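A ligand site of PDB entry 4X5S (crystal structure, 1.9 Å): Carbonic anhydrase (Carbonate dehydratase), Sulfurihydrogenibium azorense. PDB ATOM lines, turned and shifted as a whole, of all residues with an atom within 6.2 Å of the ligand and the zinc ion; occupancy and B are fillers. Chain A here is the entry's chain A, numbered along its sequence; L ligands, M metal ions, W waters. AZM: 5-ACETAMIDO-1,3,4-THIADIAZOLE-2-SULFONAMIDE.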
ATOM      1  N   SER A  37      -4.277  15.632  18.642  1.00  0.00           N
ATOM      2  CA  SER A  37      -4.184  15.239  20.043  1.00  0.00           C
ATOM      3  C   SER A  37      -2.698  15.390  20.463  1.00  0.00           C
ATOM      4  O   SER A  37      -1.797  15.340  19.628  1.00  0.00           O
ATOM      5  CB  SER A  37      -4.631  13.788  20.202  1.00  0.00           C
ATOM      6  OG  SER A  37      -6.011  13.662  19.871  1.00  0.00           O
ATOM      7  N   GLN A  74       6.907   0.345  25.180  1.00  0.00           N
ATOM      8  CA  GLN A  74       5.664  -0.194  24.675  1.00  0.00           C
ATOM      9  C   GLN A  74       5.568  -1.692  24.920  1.00  0.00           C
ATOM     10  O   GLN A  74       6.581  -2.399  24.840  1.00  0.00           O
ATOM     11  CB  GLN A  74       5.583   0.111  23.175  1.00  0.00           C
ATOM     12  CG  GLN A  74       4.362  -0.399  22.449  1.00  0.00           C
ATOM     13  CD  GLN A  74       4.416  -0.046  20.986  1.00  0.00           C
ATOM     14  OE1 GLN A  74       4.819   1.068  20.635  1.00  0.00           O
ATOM     15  NE2 GLN A  74       4.031  -0.982  20.116  1.00  0.00           N
ATOM     16  N   GLN A  94      -1.450  -2.848  21.748  1.00  0.00           N
ATOM     17  CA  GLN A  94      -0.347  -2.541  22.649  1.00  0.00           C
ATOM     18  C   GLN A  94      -0.687  -1.367  23.542  1.00  0.00           C
ATOM     19  O   GLN A  94      -1.638  -0.630  23.285  1.00  0.00           O
ATOM     20  CB  GLN A  94       0.935  -2.167  21.854  1.00  0.00           C
ATOM     21  CG  GLN A  94       0.714  -1.100  20.747  1.00  0.00           C
ATOM     22  CD  GLN A  94       1.075   0.352  21.142  1.00  0.00           C
ATOM     23  OE1 GLN A  94       1.136   0.710  22.318  1.00  0.00           O
ATOM     24  NE2 GLN A  94       1.286   1.196  20.127  1.00  0.00           N
ATOM     25  N   HIS A  96       1.477   1.796  25.873  1.00  0.00           N
ATOM     26  CA  HIS A  96       2.767   2.428  26.078  1.00  0.00           C
ATOM     27  C   HIS A  96       2.597   3.598  27.019  1.00  0.00           C
ATOM     28  O   HIS A  96       1.478   3.881  27.454  1.00  0.00           O
ATOM     29  CB  HIS A  96       3.347   2.908  24.742  1.00  0.00           C
ATOM     30  CG  HIS A  96       2.476   3.879  24.032  1.00  0.00           C
ATOM     31  ND1 HIS A  96       1.524   3.496  23.122  1.00  0.00           N
ATOM     32  CD2 HIS A  96       2.373   5.228  24.142  1.00  0.00           C
ATOM     33  CE1 HIS A  96       0.869   4.566  22.686  1.00  0.00           C
ATOM     34  NE2 HIS A  96       1.361   5.623  23.289  1.00  0.00           N
ATOM     35  N   PHE A  97       3.689   4.301  27.327  1.00  0.00           N
ATOM     36  CA  PHE A  97       3.611   5.373  28.297  1.00  0.00           C
ATOM     37  C   PHE A  97       4.215   6.724  27.925  1.00  0.00           C
ATOM     38  O   PHE A  97       5.108   6.816  27.079  1.00  0.00           O
ATOM     39  CB  PHE A  97       4.281   4.883  29.587  1.00  0.00           C
ATOM     40  CG  PHE A  97       3.646   3.644  30.156  1.00  0.00           C
ATOM     41  CD1 PHE A  97       2.710   3.741  31.186  1.00  0.00           C
ATOM     42  CD2 PHE A  97       3.968   2.393  29.659  1.00  0.00           C
ATOM     43  CE1 PHE A  97       2.103   2.589  31.712  1.00  0.00           C
ATOM     44  CE2 PHE A  97       3.368   1.243  30.192  1.00  0.00           C
ATOM     45  CZ  PHE A  97       2.429   1.350  31.221  1.00  0.00           C
ATOM     46  N   HIS A  98       3.695   7.769  28.561  1.00  0.00           N
ATOM     47  CA  HIS A  98       4.220   9.111  28.346  1.00  0.00           C
ATOM     48  C   HIS A  98       4.384   9.770  29.710  1.00  0.00           C
ATOM     49  O   HIS A  98       3.506   9.651  30.565  1.00  0.00           O
ATOM     50  CB  HIS A  98       3.271   9.968  27.505  1.00  0.00           C
ATOM     51  CG  HIS A  98       3.032   9.454  26.123  1.00  0.00           C
ATOM     52  ND1 HIS A  98       3.735   9.912  25.022  1.00  0.00           N
ATOM     53  CD2 HIS A  98       2.100   8.592  25.635  1.00  0.00           C
ATOM     54  CE1 HIS A  98       3.243   9.365  23.922  1.00  0.00           C
ATOM     55  NE2 HIS A  98       2.247   8.564  24.267  1.00  0.00           N
ATOM     56  N   GLU A 102       0.206  13.442  28.435  1.00  0.00           N
ATOM     57  CA  GLU A 102      -0.008  14.179  27.199  1.00  0.00           C
ATOM     58  C   GLU A 102      -1.268  15.036  27.375  1.00  0.00           C
ATOM     59  O   GLU A 102      -1.228  16.241  27.141  1.00  0.00           O
ATOM     60  CB  GLU A 102      -0.159  13.208  26.031  1.00  0.00           C
ATOM     61  CG  GLU A 102       1.123  12.406  25.829  1.00  0.00           C
ATOM     62  CD  GLU A 102       1.372  12.086  24.384  1.00  0.00           C
ATOM     63  OE1 GLU A 102       0.577  11.305  23.803  1.00  0.00           O
ATOM     64  OE2 GLU A 102       2.355  12.631  23.847  1.00  0.00           O
ATOM     65  N   HIS A 115      -1.340   4.685  27.366  1.00  0.00           N
ATOM     66  CA  HIS A 115      -2.183   4.610  26.181  1.00  0.00           C
ATOM     67  C   HIS A 115      -2.343   3.165  25.741  1.00  0.00           C
ATOM     68  O   HIS A 115      -1.350   2.461  25.505  1.00  0.00           O
ATOM     69  CB  HIS A 115      -1.574   5.454  25.028  1.00  0.00           C
ATOM     70  CG  HIS A 115      -1.669   6.929  25.262  1.00  0.00           C
ATOM     71  ND1 HIS A 115      -0.849   7.838  24.619  1.00  0.00           N
ATOM     72  CD2 HIS A 115      -2.477   7.664  26.061  1.00  0.00           C
ATOM     73  CE1 HIS A 115      -1.151   9.055  25.019  1.00  0.00           C
ATOM     74  NE2 HIS A 115      -2.135   8.983  25.893  1.00  0.00           N
ATOM     75  N   LEU A 116      -3.592   2.732  25.689  1.00  0.00           N
ATOM     76  CA  LEU A 116      -4.000   1.399  25.242  1.00  0.00           C
ATOM     77  C   LEU A 116      -4.441   1.604  23.789  1.00  0.00           C
ATOM     78  O   LEU A 116      -5.516   2.174  23.526  1.00  0.00           O
ATOM     79  CB  LEU A 116      -5.189   0.928  26.080  1.00  0.00           C
ATOM     80  CG  LEU A 116      -4.795   0.565  27.532  1.00  0.00           C
ATOM     81  CD1 LEU A 116      -5.967   0.803  28.489  1.00  0.00           C
ATOM     82  CD2 LEU A 116      -4.361  -0.915  27.571  1.00  0.00           C
ATOM     83  N   VAL A 117      -3.636   1.148  22.854  1.00  0.00           N
ATOM     84  CA  VAL A 117      -3.907   1.348  21.435  1.00  0.00           C
ATOM     85  C   VAL A 117      -4.637   0.164  20.795  1.00  0.00           C
ATOM     86  O   VAL A 117      -4.145  -0.950  20.810  1.00  0.00           O
ATOM     87  CB  VAL A 117      -2.572   1.605  20.685  1.00  0.00           C
ATOM     88  CG1 VAL A 117      -2.831   1.898  19.223  1.00  0.00           C
ATOM     89  CG2 VAL A 117      -1.840   2.811  21.331  1.00  0.00           C
ATOM     90  N   ILE A 125      -8.568   3.410  14.515  1.00  0.00           N
ATOM     91  CA  ILE A 125      -7.891   3.377  15.802  1.00  0.00           C
ATOM     92  C   ILE A 125      -8.674   4.002  16.964  1.00  0.00           C
ATOM     93  O   ILE A 125      -9.338   5.030  16.816  1.00  0.00           O
ATOM     94  CB  ILE A 125      -6.534   4.105  15.686  1.00  0.00           C
ATOM     95  CG1 ILE A 125      -5.680   3.412  14.607  1.00  0.00           C
ATOM     96  CG2 ILE A 125      -5.802   4.122  17.033  1.00  0.00           C
ATOM     97  CD1 ILE A 125      -4.397   4.125  14.295  1.00  0.00           C
ATOM     98  N   VAL A 127      -7.909   4.856  21.165  1.00  0.00           N
ATOM     99  CA  VAL A 127      -6.890   4.852  22.213  1.00  0.00           C
ATOM    100  C   VAL A 127      -7.556   5.189  23.547  1.00  0.00           C
ATOM    101  O   VAL A 127      -8.319   6.148  23.639  1.00  0.00           O
ATOM    102  CB  VAL A 127      -5.770   5.890  21.954  1.00  0.00           C
ATOM    103  CG1 VAL A 127      -4.702   5.789  23.058  1.00  0.00           C
ATOM    104  CG2 VAL A 127      -5.127   5.668  20.575  1.00  0.00           C
ATOM    105  N   SER A 179      -6.258  12.480  17.147  1.00  0.00           N
ATOM    106  CA  SER A 179      -5.206  11.900  16.325  1.00  0.00           C
ATOM    107  C   SER A 179      -4.189  11.108  17.104  1.00  0.00           C
ATOM    108  O   SER A 179      -4.241  11.006  18.347  1.00  0.00           O
ATOM    109  CB  SER A 179      -4.456  13.045  15.628  1.00  0.00           C
ATOM    110  OG  SER A 179      -3.550  13.664  16.533  1.00  0.00           O
ATOM    111  N   LEU A 180      -3.251  10.526  16.369  1.00  0.00           N
ATOM    112  CA  LEU A 180      -2.139   9.831  17.019  1.00  0.00           C
ATOM    113  C   LEU A 180      -1.293  11.003  17.517  1.00  0.00           C
ATOM    114  O   LEU A 180      -1.309  12.069  16.905  1.00  0.00           O
ATOM    115  CB  LEU A 180      -1.343   9.004  16.000  1.00  0.00           C
ATOM    116  CG  LEU A 180      -2.120   7.858  15.350  1.00  0.00           C
ATOM    117  CD1 LEU A 180      -1.225   7.179  14.297  1.00  0.00           C
ATOM    118  CD2 LEU A 180      -2.539   6.859  16.408  1.00  0.00           C
ATOM    119  N   THR A 181      -0.588  10.839  18.631  1.00  0.00           N
ATOM    120  CA  THR A 181       0.225  11.941  19.142  1.00  0.00           C
ATOM    121  C   THR A 181       1.697  11.907  18.719  1.00  0.00           C
ATOM    122  O   THR A 181       2.491  12.683  19.230  1.00  0.00           O
ATOM    123  CB  THR A 181       0.153  12.033  20.661  1.00  0.00           C
ATOM    124  OG1 THR A 181       0.827  10.907  21.244  1.00  0.00           O
ATOM    125  CG2 THR A 181      -1.303  12.010  21.103  1.00  0.00           C
ATOM    126  N   THR A 182       2.058  11.016  17.796  1.00  0.00           N
ATOM    127  CA  THR A 182       3.423  10.955  17.255  1.00  0.00           C
ATOM    128  C   THR A 182       3.226  10.805  15.751  1.00  0.00           C
ATOM    129  O   THR A 182       2.202  10.275  15.315  1.00  0.00           O
ATOM    130  CB  THR A 182       4.238   9.726  17.774  1.00  0.00           C
ATOM    131  OG1 THR A 182       3.655   8.530  17.282  1.00  0.00           O
ATOM    132  CG2 THR A 182       4.230   9.657  19.284  1.00  0.00           C
ATOM    133  N   PRO A 183       4.203  11.254  14.945  1.00  0.00           N
ATOM    134  CA  PRO A 183       4.101  11.163  13.485  1.00  0.00           C
ATOM    135  C   PRO A 183       3.667   9.763  13.072  1.00  0.00           C
ATOM    136  O   PRO A 183       4.110   8.797  13.672  1.00  0.00           O
ATOM    137  CB  PRO A 183       5.511  11.503  13.011  1.00  0.00           C
ATOM    138  CG  PRO A 183       5.998  12.459  14.063  1.00  0.00           C
ATOM    139  CD  PRO A 183       5.501  11.821  15.355  1.00  0.00           C
ATOM    140  N   PRO A 184       2.836   9.630  12.027  1.00  0.00           N
ATOM    141  CA  PRO A 184       2.278  10.703  11.185  1.00  0.00           C
ATOM    142  C   PRO A 184       1.103  11.528  11.725  1.00  0.00           C
ATOM    143  O   PRO A 184       0.533  12.348  10.996  1.00  0.00           O
ATOM    144  CB  PRO A 184       1.928   9.951   9.909  1.00  0.00           C
ATOM    145  CG  PRO A 184       1.446   8.654  10.432  1.00  0.00           C
ATOM    146  CD  PRO A 184       2.452   8.307  11.508  1.00  0.00           C
ATOM    147  N   VAL A 189      -8.923   9.402  14.927  1.00  0.00           N
ATOM    148  CA  VAL A 189      -8.701   8.536  16.082  1.00  0.00           C
ATOM    149  C   VAL A 189      -9.783   8.754  17.146  1.00  0.00           C
ATOM    150  O   VAL A 189     -10.156   9.892  17.425  1.00  0.00           O
ATOM    151  CB  VAL A 189      -7.311   8.806  16.749  1.00  0.00           C
ATOM    152  CG1 VAL A 189      -7.154   7.953  18.023  1.00  0.00           C
ATOM    153  CG2 VAL A 189      -6.184   8.480  15.736  1.00  0.00           C
ATOM    154  N   TRP A 191     -10.599   8.875  20.826  1.00  0.00           N
ATOM    155  CA  TRP A 191      -9.956   8.969  22.118  1.00  0.00           C
ATOM    156  C   TRP A 191     -10.975   8.753  23.252  1.00  0.00           C
ATOM    157  O   TRP A 191     -12.091   9.279  23.220  1.00  0.00           O
ATOM    158  CB  TRP A 191      -9.278  10.332  22.312  1.00  0.00           C
ATOM    159  CG  TRP A 191      -7.881  10.372  21.763  1.00  0.00           C
ATOM    160  CD1 TRP A 191      -7.498  10.809  20.524  1.00  0.00           C
ATOM    161  CD2 TRP A 191      -6.704   9.879  22.395  1.00  0.00           C
ATOM    162  NE1 TRP A 191      -6.142  10.597  20.337  1.00  0.00           N
ATOM    163  CE2 TRP A 191      -5.630  10.023  21.478  1.00  0.00           C
ATOM    164  CE3 TRP A 191      -6.445   9.311  23.659  1.00  0.00           C
ATOM    165  CZ2 TRP A 191      -4.328   9.629  21.775  1.00  0.00           C
ATOM    166  CZ3 TRP A 191      -5.153   8.925  23.962  1.00  0.00           C
ATOM    167  CH2 TRP A 191      -4.105   9.082  23.024  1.00  0.00           C
HETATM  168  C1  AZM L   1       0.199   6.861  19.198  1.00  0.00           C
HETATM  169  C2  AZM L   1       1.172   5.632  17.508  1.00  0.00           C
HETATM  170  C3  AZM L   1       1.414   3.362  16.578  1.00  0.00           C
HETATM  171  C4  AZM L   1       2.202   2.596  15.576  1.00  0.00           C
HETATM  172  N1  AZM L   1       0.357   8.226  21.511  1.00  0.00           N
HETATM  173  N2  AZM L   1       1.493   6.902  17.436  1.00  0.00           N
HETATM  174  N3  AZM L   1       0.913   7.628  18.432  1.00  0.00           N
HETATM  175  N4  AZM L   1       1.667   4.735  16.598  1.00  0.00           N
HETATM  176  O1  AZM L   1      -1.578   8.445  20.043  1.00  0.00           O
HETATM  177  O2  AZM L   1      -1.197   6.320  21.264  1.00  0.00           O
HETATM  178  O3  AZM L   1       0.617   2.863  17.336  1.00  0.00           O
HETATM  179  S1  AZM L   1      -0.677   7.479  20.589  1.00  0.00           S
HETATM  180  S2  AZM L   1       0.115   5.212  18.809  1.00  0.00           S
HETATM  181 ZN    ZN M   1       0.791   7.497  23.312  1.00  0.00          ZN
HETATM  182  O   HOH W   1       2.755   6.613  14.489  1.00  0.00           O
HETATM  183  O   HOH W   2       2.212  -0.307  17.219  1.00  0.00           O
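N of Thr 181 is in hydrogen-bond range of O1 of the ligand (3.0 Å).
The side-chain hydroxyl (OG1) of Thr 181 sits close to a nitrogen (N1) of the ligand (2.7 Å).
The side-chain hydroxyl of Thr 182 is in hydrogen-bond range of a nitrogen (N2) of the ligand (2.7 Å).
An oxygen (O3) of the ligand sits at hydrogen-bond distance from the side-chain amide nitrogen (NE2) of Gln 94, at 3.3 Å.
The side-chain amide oxygen (OE1) of Gln 94 sits at hydrogen-bond distance from a ring nitrogen (ND1) of His 96, 2.9 Å away.
ND1 of His 98 sits at hydrogen-bond distance from OE2 of Glu 102, 3.3 Å away.
O of Gln 94 is in hydrogen-bond range of N of Val 117 (2.7 Å).
The indole nitrogen (NE1) of Trp 191 is in hydrogen-bond range of the backbone carbonyl oxygen (O) of Ser 179, 2.8 Å away.
NE1 of Trp 191 lies within hydrogen-bond range of OG of Ser 37 (3.1 Å).
The side-chain carboxylate of Glu 102 lies within hydrogen-bond range of the side-chain hydroxyl of Thr 181 (2.6 Å).
Glu 102 touches the zinc ion.
Thr 181 touches the zinc ion.
The nearest printed residue that does not touch the zinc ion is Trp 191 (5.2 Å).
Water W1 lies within hydrogen-bond range of O of Pro 183 (2.7 Å) and N4 of the ligand (3.0 Å).
Water W2 bridges NE2 of Gln 94 (3.4 Å) and NE2 of Gln 74 (3.5 Å).
Merely in contact with the ligand: Glu 102 (3.8 Å), Val 117 (3.6 Å), Val 127 (3.97 Å), Leu 180 (3.4 Å) and Trp 191 (3.5 Å).
Hydrophobic or aromatic side chains within 4 Å of the ligand: His 96, His 98, His 115, Val 117, Val 127, Leu 180 and Trp 191.
The nearest printed residue that does not touch the ligand is Ser 179 (4.1 Å).
The zinc ion is bound by NE2 of His 96 (2.0 Å), N1 of the ligand (2.0 Å), NE2 of His 98 (2.0 Å) and ND1 of His 115 (2.1 Å).
The zinc ion has four donor atoms within binding distance.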
